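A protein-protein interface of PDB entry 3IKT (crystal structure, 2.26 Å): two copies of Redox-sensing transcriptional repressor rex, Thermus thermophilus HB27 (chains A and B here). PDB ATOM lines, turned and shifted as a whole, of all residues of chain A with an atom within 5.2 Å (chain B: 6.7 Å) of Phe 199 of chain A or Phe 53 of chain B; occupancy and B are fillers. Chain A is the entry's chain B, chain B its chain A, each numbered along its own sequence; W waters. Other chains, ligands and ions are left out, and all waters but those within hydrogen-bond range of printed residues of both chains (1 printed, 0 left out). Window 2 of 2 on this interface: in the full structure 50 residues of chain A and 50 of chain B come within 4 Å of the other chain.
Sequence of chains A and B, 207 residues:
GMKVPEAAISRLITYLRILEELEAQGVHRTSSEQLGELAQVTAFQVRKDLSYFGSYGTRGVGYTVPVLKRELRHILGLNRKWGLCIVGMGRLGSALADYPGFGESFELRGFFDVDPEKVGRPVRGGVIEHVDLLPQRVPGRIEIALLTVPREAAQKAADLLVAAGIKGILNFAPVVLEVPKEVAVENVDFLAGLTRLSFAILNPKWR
O of Val 4 of chain B is in hydrogen-bond range of NE1 of Trp 206 of chain A (2.7 Å).
O of Leu 76 of chain B is in hydrogen-bond range of OG of Ser 198 of chain A.
O of Gly 77 of chain B lies close to OG of Ser 198 of chain A (3.4 Å).
The indole nitrogen (NE1) of Trp 82 of chain B is in hydrogen-bond range of the side-chain hydroxyl (OG) of Ser 198 of chain A, 3.0 Å away.
The backbone carbonyl oxygen (O) of Phe 53 of chain B is in hydrogen-bond range of the side-chain hydroxyl (OH) of Tyr 56 of chain B (2.9 Å).
O of Gly 77 of chain B is in hydrogen-bond range of NE1 of Trp 82 of chain B.
The backbone carbonyl oxygen (O) of Phe 199 of chain A sits at hydrogen-bond distance from the side-chain amide nitrogen (ND2) of Asn 203 of chain A, 2.9 Å away.
Among the printed residues, merely in contact across the chains: Thr 195 of chain A with Leu 76 of chain B (3.7 Å), Phe 199 of chain A with Ile 9 of chain B (3.5 Å), Phe 199 of chain A with Phe 53 of chain B (3.8 Å), Phe 199 of chain A with Ile 75 of chain B (3.3 Å), Phe 199 of chain A with Leu 76 of chain B (3.8 Å), Ile 201 of chain A with Trp 82 of chain B (3.6 Å), Leu 202 of chain A with Gly 77 of chain B (3.4 Å) and Leu 202 of chain A with Trp 82 of chain B (3.7 Å).
Of chain B, only Ile 9, Phe 53, Ile 75 and Leu 76 come within 4 Å of Phe 199 of chain A.
Of chain A, only Phe 199 (3.8 Å) comes within 4 Å of Phe 53 of chain B.
Of the printed residues of chain B, Ser 198 of chain A touches Leu 76, Gly 77 and Trp 82.
Of the printed residues of chain B, Thr 195 of chain A touches Leu 76.
Printed residues of chain A within 4 Å of Ile 9 of chain B: Phe 199.
Of the 10 printed residues of chain A, 6 touch a printed residue of chain B.
Hydrophobic or aromatic side chains of chain A within 4 Å of the printed part of chain B: Phe 199, Ile 201, Leu 202 and Trp 206.
Along chain A the printed residues that touch a printed residue of chain B span positions 195 to 206.
Hydrophobic or aromatic side chains of chain B that line the printed part of chain A: Val 4, Ile 9, Phe 53, Leu 76 and Trp 82.
Among the printed residues, 12 pairs touch across the chains.
Among the printed residues, no Asp or Glu carboxylate lies within 4 Å of a Lys or Arg side-chain nitrogen of the other chain.
No position is printed for both chains.
Water W1 lies within hydrogen-bond range of the backbone carbonyl oxygen of Ile 75 of chain B (2.7 Å) and the side-chain amide nitrogen of Asn 203 of chain A (3.1 Å).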
ATOM      1  N   THR A 195       4.486  22.798 -14.923  1.00  0.00           N
ATOM      2  CA  THR A 195       3.187  23.371 -14.576  1.00  0.00           C
ATOM      3  C   THR A 195       3.134  23.717 -13.098  1.00  0.00           C
ATOM      4  O   THR A 195       2.533  24.715 -12.716  1.00  0.00           O
ATOM      5  CB  THR A 195       2.046  22.413 -14.937  1.00  0.00           C
ATOM      6  OG1 THR A 195       2.153  22.072 -16.325  1.00  0.00           O
ATOM      7  CG2 THR A 195       0.686  23.077 -14.712  1.00  0.00           C
ATOM      8  N   ARG A 196       3.770  22.902 -12.260  1.00  0.00           N
ATOM      9  CA  ARG A 196       3.786  23.211 -10.836  1.00  0.00           C
ATOM     10  C   ARG A 196       4.562  24.502 -10.585  1.00  0.00           C
ATOM     11  O   ARG A 196       4.204  25.277  -9.700  1.00  0.00           O
ATOM     12  CB  ARG A 196       4.389  22.060 -10.025  1.00  0.00           C
ATOM     13  CG  ARG A 196       3.463  20.845  -9.936  1.00  0.00           C
ATOM     14  CD  ARG A 196       3.801  19.975  -8.747  1.00  0.00           C
ATOM     15  NE  ARG A 196       5.121  19.379  -8.870  1.00  0.00           N
ATOM     16  CZ  ARG A 196       5.414  18.394  -9.711  1.00  0.00           C
ATOM     17  NH1 ARG A 196       4.472  17.894 -10.496  1.00  0.00           N
ATOM     18  NH2 ARG A 196       6.645  17.915  -9.775  1.00  0.00           N
ATOM     19  N   LEU A 197       5.620  24.743 -11.362  1.00  0.00           N
ATOM     20  CA  LEU A 197       6.404  25.973 -11.197  1.00  0.00           C
ATOM     21  C   LEU A 197       5.543  27.171 -11.579  1.00  0.00           C
ATOM     22  O   LEU A 197       5.615  28.231 -10.954  1.00  0.00           O
ATOM     23  CB  LEU A 197       7.667  25.959 -12.078  1.00  0.00           C
ATOM     24  CG  LEU A 197       8.901  25.205 -11.573  1.00  0.00           C
ATOM     25  CD1 LEU A 197      10.021  25.303 -12.601  1.00  0.00           C
ATOM     26  CD2 LEU A 197       9.354  25.787 -10.228  1.00  0.00           C
ATOM     27  N   SER A 198       4.736  26.993 -12.619  1.00  0.00           N
ATOM     28  CA  SER A 198       3.840  28.037 -13.082  1.00  0.00           C
ATOM     29  C   SER A 198       2.929  28.429 -11.927  1.00  0.00           C
ATOM     30  O   SER A 198       2.838  29.606 -11.557  1.00  0.00           O
ATOM     31  CB  SER A 198       2.997  27.526 -14.256  1.00  0.00           C
ATOM     32  OG  SER A 198       1.930  28.411 -14.543  1.00  0.00           O
ATOM     33  N   PHE A 199       2.269  27.431 -11.349  1.00  0.00           N
ATOM     34  CA  PHE A 199       1.365  27.678 -10.234  1.00  0.00           C
ATOM     35  C   PHE A 199       2.103  28.323  -9.068  1.00  0.00           C
ATOM     36  O   PHE A 199       1.612  29.279  -8.468  1.00  0.00           O
ATOM     37  CB  PHE A 199       0.711  26.373  -9.762  1.00  0.00           C
ATOM     38  CG  PHE A 199      -0.336  26.575  -8.704  1.00  0.00           C
ATOM     39  CD1 PHE A 199      -1.625  26.964  -9.051  1.00  0.00           C
ATOM     40  CD2 PHE A 199      -0.015  26.442  -7.359  1.00  0.00           C
ATOM     41  CE1 PHE A 199      -2.577  27.224  -8.075  1.00  0.00           C
ATOM     42  CE2 PHE A 199      -0.956  26.698  -6.371  1.00  0.00           C
ATOM     43  CZ  PHE A 199      -2.243  27.093  -6.730  1.00  0.00           C
ATOM     44  N   ALA A 200       3.288  27.805  -8.756  1.00  0.00           N
ATOM     45  CA  ALA A 200       4.085  28.324  -7.648  1.00  0.00           C
ATOM     46  C   ALA A 200       4.474  29.783  -7.844  1.00  0.00           C
ATOM     47  O   ALA A 200       4.363  30.593  -6.925  1.00  0.00           O
ATOM     48  CB  ALA A 200       5.334  27.481  -7.465  1.00  0.00           C
ATOM     49  N   ILE A 201       4.948  30.110  -9.041  1.00  0.00           N
ATOM     50  CA  ILE A 201       5.358  31.472  -9.347  1.00  0.00           C
ATOM     51  C   ILE A 201       4.164  32.429  -9.266  1.00  0.00           C
ATOM     52  O   ILE A 201       4.299  33.571  -8.830  1.00  0.00           O
ATOM     53  CB  ILE A 201       6.009  31.548 -10.756  1.00  0.00           C
ATOM     54  CG1 ILE A 201       7.342  30.783 -10.753  1.00  0.00           C
ATOM     55  CG2 ILE A 201       6.231  32.998 -11.150  1.00  0.00           C
ATOM     56  CD1 ILE A 201       7.964  30.568 -12.151  1.00  0.00           C
ATOM     57  N   LEU A 202       2.994  31.946  -9.669  1.00  0.00           N
ATOM     58  CA  LEU A 202       1.780  32.753  -9.645  1.00  0.00           C
ATOM     59  C   LEU A 202       1.188  32.859  -8.239  1.00  0.00           C
ATOM     60  O   LEU A 202       0.376  33.744  -7.962  1.00  0.00           O
ATOM     61  CB  LEU A 202       0.745  32.141 -10.590  1.00  0.00           C
ATOM     62  CG  LEU A 202       0.382  32.836 -11.901  1.00  0.00           C
ATOM     63  CD1 LEU A 202       1.531  33.661 -12.440  1.00  0.00           C
ATOM     64  CD2 LEU A 202      -0.035  31.774 -12.892  1.00  0.00           C
ATOM     65  N   ASN A 203       1.595  31.959  -7.352  1.00  0.00           N
ATOM     66  CA  ASN A 203       1.071  31.960  -5.996  1.00  0.00           C
ATOM     67  C   ASN A 203       2.184  31.986  -4.965  1.00  0.00           C
ATOM     68  O   ASN A 203       2.339  31.053  -4.181  1.00  0.00           O
ATOM     69  CB  ASN A 203       0.192  30.726  -5.792  1.00  0.00           C
ATOM     70  CG  ASN A 203      -1.078  30.774  -6.625  1.00  0.00           C
ATOM     71  OD1 ASN A 203      -2.068  31.390  -6.228  1.00  0.00           O
ATOM     72  ND2 ASN A 203      -1.049  30.138  -7.795  1.00  0.00           N
ATOM     73  N   TRP A 206       1.146  31.489  -1.166  1.00  0.00           N
ATOM     74  CA  TRP A 206       0.859  30.080  -0.919  1.00  0.00           C
ATOM     75  C   TRP A 206       2.137  29.253  -0.885  1.00  0.00           C
ATOM     76  O   TRP A 206       2.287  28.365  -0.049  1.00  0.00           O
ATOM     77  CB  TRP A 206      -0.060  29.535  -2.010  1.00  0.00           C
ATOM     78  CG  TRP A 206      -0.248  28.047  -1.966  1.00  0.00           C
ATOM     79  CD1 TRP A 206      -1.126  27.348  -1.180  1.00  0.00           C
ATOM     80  CD2 TRP A 206       0.434  27.074  -2.769  1.00  0.00           C
ATOM     81  NE1 TRP A 206      -1.035  26.003  -1.450  1.00  0.00           N
ATOM     82  CE2 TRP A 206      -0.087  25.807  -2.422  1.00  0.00           C
ATOM     83  CE3 TRP A 206       1.431  27.151  -3.749  1.00  0.00           C
ATOM     84  CZ2 TRP A 206       0.354  24.627  -3.026  1.00  0.00           C
ATOM     85  CZ3 TRP A 206       1.871  25.972  -4.351  1.00  0.00           C
ATOM     86  CH2 TRP A 206       1.330  24.728  -3.985  1.00  0.00           C
ATOM     87  N   VAL B   4      -4.854  25.137  -0.103  1.00  0.00           N
ATOM     88  CA  VAL B   4      -4.730  24.132  -1.145  1.00  0.00           C
ATOM     89  C   VAL B   4      -3.509  23.244  -0.956  1.00  0.00           C
ATOM     90  O   VAL B   4      -2.370  23.721  -0.958  1.00  0.00           O
ATOM     91  CB  VAL B   4      -4.643  24.780  -2.538  1.00  0.00           C
ATOM     92  CG1 VAL B   4      -4.686  23.702  -3.605  1.00  0.00           C
ATOM     93  CG2 VAL B   4      -5.783  25.761  -2.727  1.00  0.00           C
ATOM     94  N   ALA B   8      -2.889  18.532  -4.403  1.00  0.00           N
ATOM     95  CA  ALA B   8      -4.059  18.833  -5.235  1.00  0.00           C
ATOM     96  C   ALA B   8      -3.629  19.410  -6.584  1.00  0.00           C
ATOM     97  O   ALA B   8      -4.241  19.123  -7.613  1.00  0.00           O
ATOM     98  CB  ALA B   8      -4.978  19.821  -4.520  1.00  0.00           C
ATOM     99  N   ILE B   9      -2.576  20.222  -6.579  1.00  0.00           N
ATOM    100  CA  ILE B   9      -2.088  20.822  -7.814  1.00  0.00           C
ATOM    101  C   ILE B   9      -1.685  19.718  -8.790  1.00  0.00           C
ATOM    102  O   ILE B   9      -2.019  19.773  -9.978  1.00  0.00           O
ATOM    103  CB  ILE B   9      -0.875  21.758  -7.557  1.00  0.00           C
ATOM    104  CG1 ILE B   9      -1.245  22.826  -6.519  1.00  0.00           C
ATOM    105  CG2 ILE B   9      -0.455  22.440  -8.860  1.00  0.00           C
ATOM    106  CD1 ILE B   9      -2.495  23.643  -6.872  1.00  0.00           C
ATOM    107  N   LEU B  12      -4.723  18.292 -10.271  1.00  0.00           N
ATOM    108  CA  LEU B  12      -5.369  19.218 -11.198  1.00  0.00           C
ATOM    109  C   LEU B  12      -4.693  19.061 -12.557  1.00  0.00           C
ATOM    110  O   LEU B  12      -5.346  19.030 -13.603  1.00  0.00           O
ATOM    111  CB  LEU B  12      -5.221  20.664 -10.721  1.00  0.00           C
ATOM    112  CG  LEU B  12      -5.990  21.106  -9.480  1.00  0.00           C
ATOM    113  CD1 LEU B  12      -5.816  22.610  -9.316  1.00  0.00           C
ATOM    114  CD2 LEU B  12      -7.472  20.755  -9.626  1.00  0.00           C
ATOM    115  N   LYS B  48     -13.419  17.913  -4.349  1.00  0.00           N
ATOM    116  CA  LYS B  48     -12.739  18.648  -3.292  1.00  0.00           C
ATOM    117  C   LYS B  48     -11.603  19.505  -3.863  1.00  0.00           C
ATOM    118  O   LYS B  48     -11.417  20.659  -3.462  1.00  0.00           O
ATOM    119  CB  LYS B  48     -12.198  17.664  -2.247  1.00  0.00           C
ATOM    120  CG  LYS B  48     -11.263  18.272  -1.207  1.00  0.00           C
ATOM    121  CD  LYS B  48     -11.934  19.348  -0.364  1.00  0.00           C
ATOM    122  CE  LYS B  48     -13.045  18.772   0.515  1.00  0.00           C
ATOM    123  NZ  LYS B  48     -13.573  19.773   1.490  1.00  0.00           N
ATOM    124  N   ASP B  49     -10.849  18.944  -4.805  1.00  0.00           N
ATOM    125  CA  ASP B  49      -9.748  19.682  -5.422  1.00  0.00           C
ATOM    126  C   ASP B  49     -10.274  20.892  -6.191  1.00  0.00           C
ATOM    127  O   ASP B  49      -9.691  21.972  -6.128  1.00  0.00           O
ATOM    128  CB  ASP B  49      -8.957  18.796  -6.390  1.00  0.00           C
ATOM    129  CG  ASP B  49      -8.195  17.681  -5.689  1.00  0.00           C
ATOM    130  OD1 ASP B  49      -7.754  17.879  -4.534  1.00  0.00           O
ATOM    131  OD2 ASP B  49      -8.018  16.609  -6.312  1.00  0.00           O
ATOM    132  N   LEU B  50     -11.375  20.703  -6.918  1.00  0.00           N
ATOM    133  CA  LEU B  50     -11.964  21.780  -7.707  1.00  0.00           C
ATOM    134  C   LEU B  50     -12.527  22.873  -6.814  1.00  0.00           C
ATOM    135  O   LEU B  50     -12.298  24.062  -7.049  1.00  0.00           O
ATOM    136  CB  LEU B  50     -13.069  21.237  -8.617  1.00  0.00           C
ATOM    137  CG  LEU B  50     -12.672  20.206  -9.678  1.00  0.00           C
ATOM    138  CD1 LEU B  50     -13.876  19.921 -10.555  1.00  0.00           C
ATOM    139  CD2 LEU B  50     -11.516  20.733 -10.535  1.00  0.00           C
ATOM    140  N   SER B  51     -13.249  22.461  -5.779  1.00  0.00           N
ATOM    141  CA  SER B  51     -13.859  23.398  -4.841  1.00  0.00           C
ATOM    142  C   SER B  51     -12.856  24.383  -4.253  1.00  0.00           C
ATOM    143  O   SER B  51     -13.234  25.481  -3.839  1.00  0.00           O
ATOM    144  CB  SER B  51     -14.554  22.642  -3.707  1.00  0.00           C
ATOM    145  OG  SER B  51     -13.618  22.123  -2.786  1.00  0.00           O
ATOM    146  N   TYR B  52     -11.584  23.998  -4.199  1.00  0.00           N
ATOM    147  CA  TYR B  52     -10.566  24.902  -3.664  1.00  0.00           C
ATOM    148  C   TYR B  52     -10.568  26.194  -4.472  1.00  0.00           C
ATOM    149  O   TYR B  52     -10.328  27.273  -3.938  1.00  0.00           O
ATOM    150  CB  TYR B  52      -9.167  24.283  -3.758  1.00  0.00           C
ATOM    151  CG  TYR B  52      -8.900  23.195  -2.755  1.00  0.00           C
ATOM    152  CD1 TYR B  52      -8.342  21.984  -3.153  1.00  0.00           C
ATOM    153  CD2 TYR B  52      -9.234  23.360  -1.410  1.00  0.00           C
ATOM    154  CE1 TYR B  52      -8.131  20.958  -2.240  1.00  0.00           C
ATOM    155  CE2 TYR B  52      -9.028  22.340  -0.488  1.00  0.00           C
ATOM    156  CZ  TYR B  52      -8.479  21.141  -0.912  1.00  0.00           C
ATOM    157  OH  TYR B  52      -8.305  20.116  -0.015  1.00  0.00           O
ATOM    158  N   PHE B  53     -10.854  26.077  -5.762  1.00  0.00           N
ATOM    159  CA  PHE B  53     -10.839  27.237  -6.627  1.00  0.00           C
ATOM    160  C   PHE B  53     -12.198  27.770  -7.065  1.00  0.00           C
ATOM    161  O   PHE B  53     -12.309  28.927  -7.460  1.00  0.00           O
ATOM    162  CB  PHE B  53      -9.967  26.941  -7.852  1.00  0.00           C
ATOM    163  CG  PHE B  53      -8.559  26.547  -7.501  1.00  0.00           C
ATOM    164  CD1 PHE B  53      -8.239  25.219  -7.235  1.00  0.00           C
ATOM    165  CD2 PHE B  53      -7.564  27.513  -7.387  1.00  0.00           C
ATOM    166  CE1 PHE B  53      -6.941  24.856  -6.857  1.00  0.00           C
ATOM    167  CE2 PHE B  53      -6.262  27.164  -7.008  1.00  0.00           C
ATOM    168  CZ  PHE B  53      -5.952  25.833  -6.743  1.00  0.00           C
ATOM    169  N   GLY B  54     -13.233  26.946  -7.001  1.00  0.00           N
ATOM    170  CA  GLY B  54     -14.534  27.438  -7.411  1.00  0.00           C
ATOM    171  C   GLY B  54     -15.570  26.381  -7.703  1.00  0.00           C
ATOM    172  O   GLY B  54     -15.371  25.198  -7.435  1.00  0.00           O
ATOM    173  N   SER B  55     -16.693  26.826  -8.255  1.00  0.00           N
ATOM    174  CA  SER B  55     -17.792  25.940  -8.604  1.00  0.00           C
ATOM    175  C   SER B  55     -17.930  25.988 -10.119  1.00  0.00           C
ATOM    176  O   SER B  55     -18.596  26.865 -10.666  1.00  0.00           O
ATOM    177  CB  SER B  55     -19.080  26.425  -7.932  1.00  0.00           C
ATOM    178  OG  SER B  55     -18.872  26.656  -6.544  1.00  0.00           O
ATOM    179  N   TYR B  56     -17.293  25.039 -10.796  1.00  0.00           N
ATOM    180  CA  TYR B  56     -17.319  25.003 -12.251  1.00  0.00           C
ATOM    181  C   TYR B  56     -18.316  23.990 -12.784  1.00  0.00           C
ATOM    182  O   TYR B  56     -18.497  23.865 -13.995  1.00  0.00           O
ATOM    183  CB  TYR B  56     -15.916  24.691 -12.782  1.00  0.00           C
ATOM    184  CG  TYR B  56     -14.834  25.507 -12.113  1.00  0.00           C
ATOM    185  CD1 TYR B  56     -13.953  24.924 -11.201  1.00  0.00           C
ATOM    186  CD2 TYR B  56     -14.724  26.875 -12.350  1.00  0.00           C
ATOM    187  CE1 TYR B  56     -12.992  25.686 -10.541  1.00  0.00           C
ATOM    188  CE2 TYR B  56     -13.769  27.645 -11.695  1.00  0.00           C
ATOM    189  CZ  TYR B  56     -12.906  27.048 -10.790  1.00  0.00           C
ATOM    190  OH  TYR B  56     -11.975  27.820 -10.125  1.00  0.00           O
ATOM    191  N   GLU B  71     -10.974  26.447 -17.204  1.00  0.00           N
ATOM    192  CA  GLU B  71     -10.796  26.875 -15.818  1.00  0.00           C
ATOM    193  C   GLU B  71      -9.514  26.323 -15.199  1.00  0.00           C
ATOM    194  O   GLU B  71      -8.860  26.995 -14.403  1.00  0.00           O
ATOM    195  CB  GLU B  71     -11.999  26.437 -14.966  1.00  0.00           C
ATOM    196  CG  GLU B  71     -13.350  26.943 -15.464  1.00  0.00           C
ATOM    197  CD  GLU B  71     -13.486  28.455 -15.393  1.00  0.00           C
ATOM    198  OE1 GLU B  71     -14.450  28.991 -15.982  1.00  0.00           O
ATOM    199  OE2 GLU B  71     -12.638  29.109 -14.748  1.00  0.00           O
ATOM    200  N   LEU B  72      -9.153  25.098 -15.566  1.00  0.00           N
ATOM    201  CA  LEU B  72      -7.954  24.484 -15.015  1.00  0.00           C
ATOM    202  C   LEU B  72      -6.649  25.064 -15.564  1.00  0.00           C
ATOM    203  O   LEU B  72      -5.747  25.405 -14.796  1.00  0.00           O
ATOM    204  CB  LEU B  72      -7.990  22.965 -15.226  1.00  0.00           C
ATOM    205  CG  LEU B  72      -9.038  22.206 -14.406  1.00  0.00           C
ATOM    206  CD1 LEU B  72      -8.790  20.720 -14.554  1.00  0.00           C
ATOM    207  CD2 LEU B  72      -8.964  22.603 -12.926  1.00  0.00           C
ATOM    208  N   HIS B  74      -6.233  27.753 -16.480  1.00  0.00           N
ATOM    209  CA  HIS B  74      -6.205  29.122 -15.986  1.00  0.00           C
ATOM    210  C   HIS B  74      -5.662  29.076 -14.562  1.00  0.00           C
ATOM    211  O   HIS B  74      -4.768  29.838 -14.189  1.00  0.00           O
ATOM    212  CB  HIS B  74      -7.614  29.723 -15.990  1.00  0.00           C
ATOM    213  CG  HIS B  74      -7.708  31.032 -15.271  1.00  0.00           C
ATOM    214  ND1 HIS B  74      -6.970  32.136 -15.638  1.00  0.00           N
ATOM    215  CD2 HIS B  74      -8.427  31.405 -14.186  1.00  0.00           C
ATOM    216  CE1 HIS B  74      -7.227  33.132 -14.810  1.00  0.00           C
ATOM    217  NE2 HIS B  74      -8.108  32.715 -13.920  1.00  0.00           N
ATOM    218  N   ILE B  75      -6.218  28.177 -13.761  1.00  0.00           N
ATOM    219  CA  ILE B  75      -5.774  28.019 -12.384  1.00  0.00           C
ATOM    220  C   ILE B  75      -4.286  27.669 -12.355  1.00  0.00           C
ATOM    221  O   ILE B  75      -3.536  28.165 -11.517  1.00  0.00           O
ATOM    222  CB  ILE B  75      -6.566  26.895 -11.683  1.00  0.00           C
ATOM    223  CG1 ILE B  75      -8.029  27.322 -11.516  1.00  0.00           C
ATOM    224  CG2 ILE B  75      -5.930  26.569 -10.335  1.00  0.00           C
ATOM    225  CD1 ILE B  75      -8.952  26.220 -11.030  1.00  0.00           C
ATOM    226  N   LEU B  76      -3.868  26.821 -13.288  1.00  0.00           N
ATOM    227  CA  LEU B  76      -2.483  26.380 -13.363  1.00  0.00           C
ATOM    228  C   LEU B  76      -1.524  27.380 -14.024  1.00  0.00           C
ATOM    229  O   LEU B  76      -0.316  27.131 -14.101  1.00  0.00           O
ATOM    230  CB  LEU B  76      -2.429  25.028 -14.077  1.00  0.00           C
ATOM    231  CG  LEU B  76      -3.172  23.921 -13.316  1.00  0.00           C
ATOM    232  CD1 LEU B  76      -3.268  22.661 -14.173  1.00  0.00           C
ATOM    233  CD2 LEU B  76      -2.439  23.634 -12.003  1.00  0.00           C
ATOM    234  N   GLY B  77      -2.065  28.505 -14.493  1.00  0.00           N
ATOM    235  CA  GLY B  77      -1.243  29.528 -15.122  1.00  0.00           C
ATOM    236  C   GLY B  77      -0.835  29.214 -16.547  1.00  0.00           C
ATOM    237  O   GLY B  77       0.101  29.808 -17.082  1.00  0.00           O
ATOM    238  N   TRP B  82       4.992  31.431 -20.845  1.00  0.00           N
ATOM    239  CA  TRP B  82       6.145  31.522 -19.959  1.00  0.00           C
ATOM    240  C   TRP B  82       7.426  31.477 -20.765  1.00  0.00           C
ATOM    241  O   TRP B  82       7.528  30.732 -21.735  1.00  0.00           O
ATOM    242  CB  TRP B  82       6.175  30.356 -18.958  1.00  0.00           C
ATOM    243  CG  TRP B  82       5.100  30.370 -17.922  1.00  0.00           C
ATOM    244  CD1 TRP B  82       3.915  29.699 -17.963  1.00  0.00           C
ATOM    245  CD2 TRP B  82       5.109  31.098 -16.689  1.00  0.00           C
ATOM    246  NE1 TRP B  82       3.183  29.962 -16.829  1.00  0.00           N
ATOM    247  CE2 TRP B  82       3.891  30.819 -16.031  1.00  0.00           C
ATOM    248  CE3 TRP B  82       6.032  31.959 -16.075  1.00  0.00           C
ATOM    249  CZ2 TRP B  82       3.566  31.373 -14.784  1.00  0.00           C
ATOM    250  CZ3 TRP B  82       5.711  32.509 -14.837  1.00  0.00           C
ATOM    251  CH2 TRP B  82       4.485  32.212 -14.206  1.00  0.00           C
HETATM  252  O   HOH W   1      -3.373  30.219  -9.780  1.00  0.00           O
